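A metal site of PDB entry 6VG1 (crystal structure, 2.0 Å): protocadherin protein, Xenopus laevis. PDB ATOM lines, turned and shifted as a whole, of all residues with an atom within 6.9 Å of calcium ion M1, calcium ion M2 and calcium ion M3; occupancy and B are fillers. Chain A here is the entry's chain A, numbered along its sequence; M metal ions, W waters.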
ATOM      1  N   GLU A 114     -23.532   2.214  -3.445  1.00  0.00           N
ATOM      2  CA  GLU A 114     -24.739   1.448  -3.137  1.00  0.00           C
ATOM      3  C   GLU A 114     -25.863   2.354  -2.652  1.00  0.00           C
ATOM      4  O   GLU A 114     -27.027   1.929  -2.638  1.00  0.00           O
ATOM      5  CB  GLU A 114     -24.443   0.373  -2.096  1.00  0.00           C
ATOM      6  CG  GLU A 114     -24.407   0.848  -0.664  1.00  0.00           C
ATOM      7  CD  GLU A 114     -24.097  -0.301   0.286  1.00  0.00           C
ATOM      8  OE1 GLU A 114     -24.870  -1.287   0.309  1.00  0.00           O
ATOM      9  OE2 GLU A 114     -23.065  -0.221   0.999  1.00  0.00           O
ATOM     10  N   LEU A 170     -29.209  -0.655  -4.974  1.00  0.00           N
ATOM     11  CA  LEU A 170     -28.081  -1.565  -4.840  1.00  0.00           C
ATOM     12  C   LEU A 170     -27.823  -1.917  -3.372  1.00  0.00           C
ATOM     13  O   LEU A 170     -28.226  -1.197  -2.462  1.00  0.00           O
ATOM     14  CB  LEU A 170     -26.805  -0.976  -5.442  1.00  0.00           C
ATOM     15  CG  LEU A 170     -26.780  -0.775  -6.950  1.00  0.00           C
ATOM     16  CD1 LEU A 170     -25.458  -0.132  -7.329  1.00  0.00           C
ATOM     17  CD2 LEU A 170     -26.996  -2.055  -7.714  1.00  0.00           C
ATOM     18  N   ASP A 171     -27.120  -3.039  -3.165  1.00  0.00           N
ATOM     19  CA  ASP A 171     -26.673  -3.468  -1.838  1.00  0.00           C
ATOM     20  C   ASP A 171     -25.324  -4.140  -2.036  1.00  0.00           C
ATOM     21  O   ASP A 171     -25.258  -5.291  -2.477  1.00  0.00           O
ATOM     22  CB  ASP A 171     -27.688  -4.409  -1.188  1.00  0.00           C
ATOM     23  CG  ASP A 171     -27.266  -4.824   0.217  1.00  0.00           C
ATOM     24  OD1 ASP A 171     -26.281  -4.259   0.747  1.00  0.00           O
ATOM     25  OD2 ASP A 171     -27.947  -5.709   0.796  1.00  0.00           O
ATOM     26  N   ARG A 172     -24.249  -3.436  -1.656  1.00  0.00           N
ATOM     27  CA  ARG A 172     -22.910  -3.990  -1.875  1.00  0.00           C
ATOM     28  C   ARG A 172     -22.680  -5.266  -1.085  1.00  0.00           C
ATOM     29  O   ARG A 172     -21.849  -6.092  -1.479  1.00  0.00           O
ATOM     30  CB  ARG A 172     -21.843  -2.946  -1.516  1.00  0.00           C
ATOM     31  CG  ARG A 172     -20.457  -3.298  -2.037  1.00  0.00           C
ATOM     32  CD  ARG A 172     -19.347  -2.664  -1.208  1.00  0.00           C
ATOM     33  NE  ARG A 172     -19.339  -3.178   0.167  1.00  0.00           N
ATOM     34  CZ  ARG A 172     -18.634  -4.235   0.560  1.00  0.00           C
ATOM     35  NH1 ARG A 172     -17.871  -4.897  -0.292  1.00  0.00           N
ATOM     36  NH2 ARG A 172     -18.690  -4.619   1.825  1.00  0.00           N
ATOM     37  N   GLU A 173     -23.379  -5.451   0.034  1.00  0.00           N
ATOM     38  CA  GLU A 173     -23.199  -6.656   0.829  1.00  0.00           C
ATOM     39  C   GLU A 173     -23.809  -7.877   0.142  1.00  0.00           C
ATOM     40  O   GLU A 173     -23.336  -8.994   0.336  1.00  0.00           O
ATOM     41  CB  GLU A 173     -23.795  -6.454   2.219  1.00  0.00           C
ATOM     42  CG  GLU A 173     -22.976  -5.515   3.124  1.00  0.00           C
ATOM     43  CD  GLU A 173     -22.871  -4.093   2.591  1.00  0.00           C
ATOM     44  OE1 GLU A 173     -23.808  -3.637   1.914  1.00  0.00           O
ATOM     45  OE2 GLU A 173     -21.835  -3.436   2.856  1.00  0.00           O
ATOM     46  N   SER A 174     -24.871  -7.678  -0.659  1.00  0.00           N
ATOM     47  CA  SER A 174     -25.424  -8.753  -1.466  1.00  0.00           C
ATOM     48  C   SER A 174     -24.608  -8.972  -2.734  1.00  0.00           C
ATOM     49  O   SER A 174     -24.263 -10.106  -3.077  1.00  0.00           O
ATOM     50  CB  SER A 174     -26.885  -8.452  -1.833  1.00  0.00           C
ATOM     51  OG  SER A 174     -27.731  -8.448  -0.698  1.00  0.00           O
ATOM     52  N   LEU A 203     -19.546   0.842  -4.798  1.00  0.00           N
ATOM     53  CA  LEU A 203     -18.795   1.454  -3.722  1.00  0.00           C
ATOM     54  C   LEU A 203     -19.589   1.416  -2.427  1.00  0.00           C
ATOM     55  O   LEU A 203     -20.809   1.598  -2.430  1.00  0.00           O
ATOM     56  CB  LEU A 203     -18.452   2.908  -4.065  1.00  0.00           C
ATOM     57  CG  LEU A 203     -17.648   3.103  -5.352  1.00  0.00           C
ATOM     58  CD1 LEU A 203     -17.407   4.589  -5.578  1.00  0.00           C
ATOM     59  CD2 LEU A 203     -16.339   2.352  -5.310  1.00  0.00           C
ATOM     60  N   ASP A 204     -18.889   1.174  -1.312  1.00  0.00           N
ATOM     61  CA  ASP A 204     -19.581   0.872  -0.068  1.00  0.00           C
ATOM     62  C   ASP A 204     -20.076   2.137   0.623  1.00  0.00           C
ATOM     63  O   ASP A 204     -19.403   3.178   0.611  1.00  0.00           O
ATOM     64  CB  ASP A 204     -18.693   0.092   0.893  1.00  0.00           C
ATOM     65  CG  ASP A 204     -19.437  -0.340   2.157  1.00  0.00           C
ATOM     66  OD1 ASP A 204     -20.321  -1.210   2.056  1.00  0.00           O
ATOM     67  OD2 ASP A 204     -19.116   0.184   3.250  1.00  0.00           O
ATOM     68  N   PHE A 205     -21.257   2.039   1.209  1.00  0.00           N
ATOM     69  CA  PHE A 205     -21.806   3.004   2.147  1.00  0.00           C
ATOM     70  C   PHE A 205     -21.891   2.322   3.504  1.00  0.00           C
ATOM     71  O   PHE A 205     -22.000   1.092   3.585  1.00  0.00           O
ATOM     72  CB  PHE A 205     -23.181   3.481   1.672  1.00  0.00           C
ATOM     73  CG  PHE A 205     -23.780   4.560   2.525  1.00  0.00           C
ATOM     74  CD1 PHE A 205     -23.151   5.791   2.672  1.00  0.00           C
ATOM     75  CD2 PHE A 205     -24.987   4.358   3.157  1.00  0.00           C
ATOM     76  CE1 PHE A 205     -23.709   6.780   3.453  1.00  0.00           C
ATOM     77  CE2 PHE A 205     -25.554   5.342   3.936  1.00  0.00           C
ATOM     78  CZ  PHE A 205     -24.915   6.554   4.084  1.00  0.00           C
ATOM     79  N   ASN A 206     -21.805   3.113   4.574  1.00  0.00           N
ATOM     80  CA  ASN A 206     -21.858   2.567   5.934  1.00  0.00           C
ATOM     81  C   ASN A 206     -23.318   2.492   6.382  1.00  0.00           C
ATOM     82  O   ASN A 206     -23.790   3.276   7.197  1.00  0.00           O
ATOM     83  CB  ASN A 206     -21.024   3.408   6.890  1.00  0.00           C
ATOM     84  CG  ASN A 206     -20.926   2.784   8.271  1.00  0.00           C
ATOM     85  OD1 ASN A 206     -20.696   1.581   8.413  1.00  0.00           O
ATOM     86  ND2 ASN A 206     -21.120   3.601   9.294  1.00  0.00           N
ATOM     87  N   ASP A 207     -24.025   1.521   5.802  1.00  0.00           N
ATOM     88  CA  ASP A 207     -25.430   1.305   6.088  1.00  0.00           C
ATOM     89  C   ASP A 207     -25.668   0.092   6.966  1.00  0.00           C
ATOM     90  O   ASP A 207     -26.817  -0.352   7.102  1.00  0.00           O
ATOM     91  CB  ASP A 207     -26.204   1.156   4.777  1.00  0.00           C
ATOM     92  CG  ASP A 207     -25.562   0.143   3.844  1.00  0.00           C
ATOM     93  OD1 ASP A 207     -24.368  -0.184   4.028  1.00  0.00           O
ATOM     94  OD2 ASP A 207     -26.265  -0.311   2.900  1.00  0.00           O
ATOM     95  N   ASN A 208     -24.624  -0.438   7.595  1.00  0.00           N
ATOM     96  CA  ASN A 208     -24.764  -1.549   8.521  1.00  0.00           C
ATOM     97  C   ASN A 208     -24.040  -1.226   9.805  1.00  0.00           C
ATOM     98  O   ASN A 208     -22.816  -1.089   9.825  1.00  0.00           O
ATOM     99  CB  ASN A 208     -24.225  -2.842   7.899  1.00  0.00           C
ATOM    100  CG  ASN A 208     -25.168  -3.425   6.888  1.00  0.00           C
ATOM    101  OD1 ASN A 208     -24.892  -3.433   5.693  1.00  0.00           O
ATOM    102  ND2 ASN A 208     -26.306  -3.914   7.368  1.00  0.00           N
ATOM    103  N   SER A 209     -24.790  -1.147  10.903  1.00  0.00           N
ATOM    104  CA  SER A 209     -24.195  -1.007  12.207  1.00  0.00           C
ATOM    105  C   SER A 209     -23.614  -2.349  12.631  1.00  0.00           C
ATOM    106  O   SER A 209     -24.066  -3.399  12.168  1.00  0.00           O
ATOM    107  CB  SER A 209     -25.246  -0.569  13.212  1.00  0.00           C
ATOM    108  OG  SER A 209     -26.447  -1.296  12.973  1.00  0.00           O
ATOM    109  N   PRO A 210     -22.603  -2.344  13.498  1.00  0.00           N
ATOM    110  CA  PRO A 210     -22.074  -3.622  14.000  1.00  0.00           C
ATOM    111  C   PRO A 210     -23.140  -4.373  14.793  1.00  0.00           C
ATOM    112  O   PRO A 210     -24.174  -3.815  15.175  1.00  0.00           O
ATOM    113  CB  PRO A 210     -20.898  -3.216  14.899  1.00  0.00           C
ATOM    114  CG  PRO A 210     -21.044  -1.740  15.115  1.00  0.00           C
ATOM    115  CD  PRO A 210     -21.830  -1.183  13.966  1.00  0.00           C
ATOM    116  N   ASP A 238     -19.204  -6.636  11.472  1.00  0.00           N
ATOM    117  CA  ASP A 238     -19.769  -5.565  10.651  1.00  0.00           C
ATOM    118  C   ASP A 238     -19.603  -5.972   9.188  1.00  0.00           C
ATOM    119  O   ASP A 238     -18.468  -6.208   8.749  1.00  0.00           O
ATOM    120  CB  ASP A 238     -19.069  -4.230  10.904  1.00  0.00           C
ATOM    121  CG  ASP A 238     -19.879  -3.033  10.402  1.00  0.00           C
ATOM    122  OD1 ASP A 238     -20.394  -2.264  11.239  1.00  0.00           O
ATOM    123  OD2 ASP A 238     -19.975  -2.858   9.169  1.00  0.00           O
ATOM    124  N   PRO A 239     -20.677  -6.077   8.419  1.00  0.00           N
ATOM    125  CA  PRO A 239     -20.528  -6.548   7.023  1.00  0.00           C
ATOM    126  C   PRO A 239     -19.907  -5.518   6.093  1.00  0.00           C
ATOM    127  O   PRO A 239     -19.431  -5.903   5.023  1.00  0.00           O
ATOM    128  CB  PRO A 239     -21.967  -6.891   6.613  1.00  0.00           C
ATOM    129  CG  PRO A 239     -22.814  -5.967   7.443  1.00  0.00           C
ATOM    130  CD  PRO A 239     -22.096  -5.829   8.769  1.00  0.00           C
ATOM    131  N   ASP A 240     -19.899  -4.240   6.477  1.00  0.00           N
ATOM    132  CA  ASP A 240     -19.408  -3.181   5.593  1.00  0.00           C
ATOM    133  C   ASP A 240     -17.925  -3.398   5.295  1.00  0.00           C
ATOM    134  O   ASP A 240     -17.262  -4.254   5.865  1.00  0.00           O
ATOM    135  CB  ASP A 240     -19.626  -1.806   6.234  1.00  0.00           C
ATOM    136  CG  ASP A 240     -21.113  -1.417   6.373  1.00  0.00           C
ATOM    137  OD1 ASP A 240     -21.518  -1.014   7.491  1.00  0.00           O
ATOM    138  OD2 ASP A 240     -21.876  -1.508   5.374  1.00  0.00           O
ATOM    139  N   GLU A 241     -17.406  -2.562   4.391  1.00  0.00           N
ATOM    140  CA  GLU A 241     -16.067  -2.735   3.829  1.00  0.00           C
ATOM    141  C   GLU A 241     -15.067  -1.835   4.539  1.00  0.00           C
ATOM    142  O   GLU A 241     -15.395  -0.739   4.989  1.00  0.00           O
ATOM    143  CB  GLU A 241     -16.054  -2.425   2.327  1.00  0.00           C
ATOM    144  CG  GLU A 241     -14.689  -2.566   1.680  1.00  0.00           C
ATOM    145  CD  GLU A 241     -14.699  -2.160   0.210  1.00  0.00           C
ATOM    146  OE1 GLU A 241     -15.807  -2.019  -0.375  1.00  0.00           O
ATOM    147  OE2 GLU A 241     -13.610  -1.974  -0.375  1.00  0.00           O
ATOM    148  N   ALA A 243     -12.844   0.432   6.570  1.00  0.00           N
ATOM    149  CA  ALA A 243     -13.019   1.118   7.849  1.00  0.00           C
ATOM    150  C   ALA A 243     -14.471   1.038   8.326  1.00  0.00           C
ATOM    151  O   ALA A 243     -14.730   0.944   9.526  1.00  0.00           O
ATOM    152  CB  ALA A 243     -12.582   2.579   7.724  1.00  0.00           C
ATOM    153  N   ASN A 244     -15.428   1.090   7.400  1.00  0.00           N
ATOM    154  CA  ASN A 244     -16.824   1.023   7.803  1.00  0.00           C
ATOM    155  C   ASN A 244     -17.182  -0.278   8.510  1.00  0.00           C
ATOM    156  O   ASN A 244     -18.237  -0.370   9.128  1.00  0.00           O
ATOM    157  CB  ASN A 244     -17.748   1.186   6.596  1.00  0.00           C
ATOM    158  CG  ASN A 244     -17.638   2.565   5.989  1.00  0.00           C
ATOM    159  OD1 ASN A 244     -17.111   3.484   6.615  1.00  0.00           O
ATOM    160  ND2 ASN A 244     -18.135   2.726   4.778  1.00  0.00           N
ATOM    161  N   GLY A 245     -16.311  -1.286   8.438  1.00  0.00           N
ATOM    162  CA  GLY A 245     -16.578  -2.563   9.046  1.00  0.00           C
ATOM    163  C   GLY A 245     -15.570  -2.919  10.127  1.00  0.00           C
ATOM    164  O   GLY A 245     -15.575  -4.041  10.648  1.00  0.00           O
ATOM    165  N   GLU A 246     -14.686  -1.969  10.443  1.00  0.00           N
ATOM    166  CA  GLU A 246     -13.649  -2.166  11.445  1.00  0.00           C
ATOM    167  C   GLU A 246     -14.177  -1.673  12.787  1.00  0.00           C
ATOM    168  O   GLU A 246     -14.595  -0.512  12.895  1.00  0.00           O
ATOM    169  CB  GLU A 246     -12.372  -1.423  11.037  1.00  0.00           C
ATOM    170  CG  GLU A 246     -11.108  -1.882  11.749  1.00  0.00           C
ATOM    171  CD  GLU A 246      -9.841  -1.309  11.126  1.00  0.00           C
ATOM    172  OE1 GLU A 246      -9.945  -0.593  10.104  1.00  0.00           O
ATOM    173  OE2 GLU A 246      -8.744  -1.585  11.657  1.00  0.00           O
ATOM    174  N   ASP A 294     -18.174   1.121  14.630  1.00  0.00           N
ATOM    175  CA  ASP A 294     -17.334   1.045  13.441  1.00  0.00           C
ATOM    176  C   ASP A 294     -16.615   2.376  13.231  1.00  0.00           C
ATOM    177  O   ASP A 294     -17.079   3.428  13.673  1.00  0.00           O
ATOM    178  CB  ASP A 294     -18.135   0.676  12.190  1.00  0.00           C
ATOM    179  CG  ASP A 294     -19.255   1.652  11.877  1.00  0.00           C
ATOM    180  OD1 ASP A 294     -19.294   2.747  12.473  1.00  0.00           O
ATOM    181  OD2 ASP A 294     -20.105   1.303  11.033  1.00  0.00           O
ATOM    182  N   MET A 295     -15.477   2.318  12.538  1.00  0.00           N
ATOM    183  CA  MET A 295     -14.666   3.508  12.302  1.00  0.00           C
ATOM    184  C   MET A 295     -15.010   4.070  10.929  1.00  0.00           C
ATOM    185  O   MET A 295     -14.302   3.891   9.936  1.00  0.00           O
ATOM    186  CB  MET A 295     -13.188   3.168  12.433  1.00  0.00           C
ATOM    187  CG  MET A 295     -12.782   2.866  13.852  1.00  0.00           C
ATOM    188  SD  MET A 295     -11.027   2.512  14.011  1.00  0.00           S
ATOM    189  CE  MET A 295     -10.970   0.892  13.225  1.00  0.00           C
ATOM    190  N   ALA A 296     -16.149   4.760  10.885  1.00  0.00           N
ATOM    191  CA  ALA A 296     -16.644   5.367   9.659  1.00  0.00           C
ATOM    192  C   ALA A 296     -16.934   6.842   9.903  1.00  0.00           C
ATOM    193  O   ALA A 296     -16.960   7.327  11.043  1.00  0.00           O
ATOM    194  CB  ALA A 296     -17.905   4.660   9.147  1.00  0.00           C
ATOM    195  N   LEU A 300     -21.535   3.909  13.420  1.00  0.00           N
ATOM    196  CA  LEU A 300     -22.674   3.122  13.875  1.00  0.00           C
ATOM    197  C   LEU A 300     -22.255   2.291  15.080  1.00  0.00           C
ATOM    198  O   LEU A 300     -21.095   1.898  15.218  1.00  0.00           O
ATOM    199  CB  LEU A 300     -23.177   2.230  12.752  1.00  0.00           C
ATOM    200  CG  LEU A 300     -23.613   3.021  11.509  1.00  0.00           C
ATOM    201  CD1 LEU A 300     -23.921   2.161  10.320  1.00  0.00           C
ATOM    202  CD2 LEU A 300     -24.824   3.892  11.910  1.00  0.00           C
HETATM  203 CA    CA M   1     -20.570  -0.529   9.612  1.00  0.00          CA
HETATM  204 CA    CA M   2     -22.461  -1.221   3.050  1.00  0.00          CA
HETATM  205 CA    CA M   3     -25.707  -2.315   2.145  1.00  0.00          CA
HETATM  206  O   HOH W   1     -27.656  -2.101   1.022  1.00  0.00           O
HETATM  207  O   HOH W   2     -27.003  -3.873   3.773  1.00  0.00           O
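The backbone NH (N) of Arg 172 lies close to the side-chain carboxylate (OE1) of Glu 114, at 3.0 Å.
The side-chain carboxylate (OD2) of Asp 204 sits at hydrogen-bond distance from the backbone NH (N) of Glu 241.
OD2 of Asp 171 sits at hydrogen-bond distance from OG of Ser 174, 3.1 Å away.
The backbone NH of Glu 114 lies within hydrogen-bond range of the backbone carbonyl oxygen of Leu 203 (3.0 Å).
The side-chain amide nitrogen of Asn 244 lies within hydrogen-bond range of the side-chain carboxylate of Asp 204.
OD1 of Asp 294 sits at hydrogen-bond distance from N of Leu 300, at 2.7 Å.
OE2 of Glu 173 sits close to NH2 of Arg 172 (3.5 Å).
The side-chain carboxylate of Asp 204 lies close to the guanidinium group of Arg 172 (2.9 Å).
Within 4 Å of calcium ion M2: Glu 114, Glu 173, Asp 204, Phe 205, Asp 207 and Asp 240.
Five residues have an atom within 4 Å of calcium ion M3: Glu 114, Asp 171, Glu 173, Asp 207 and Asn 208.
The nearest printed residue that does not touch calcium ion M3 is Arg 172 (4.2 Å).
Calcium ion M1 is bound by O of Asn 208 (2.3 Å), OD2 of Asp 294 (2.4 Å), OD1 of Asp 240 (2.4 Å), OD1 of Asp 238 (2.4 Å), O of Asn 244 (2.4 Å), OD1 of Asn 206 (2.4 Å) and OD2 of Asp 238 (2.4 Å).
Calcium ion M1 has seven donor atoms within binding distance.
Calcium ion M2 is bound by the side-chain carboxylate of Glu 173 (2.3 Å), the side-chain carboxylate of Glu 114 (2.4 Å), the side-chain carboxylate of Asp 204 (2.4 Å), the side-chain carboxylate of Asp 207 (2.4 Å), the side-chain carboxylate of Asp 240 (2.4 Å) and the backbone carbonyl oxygen of Phe 205 (2.4 Å).
Calcium ion M2 has six donor atoms within binding distance.
Slightly farther from calcium ion M2 lies OE1 of Glu 173 (3.0 Å).
Calcium ion M3 is bound by the side-chain carboxylate of Asp 207 (2.2 Å), water W1 (2.3 Å), the side-chain carboxylate of Glu 114 (2.3 Å), the side-chain carboxylate of Glu 173 (2.3 Å), the side-chain carboxylate of Asp 171 (2.5 Å) and water W2 (2.6 Å).
Slightly farther from calcium ion M3 lies the side-chain carboxylate (OD1) of Asp 207 (3.1 Å).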
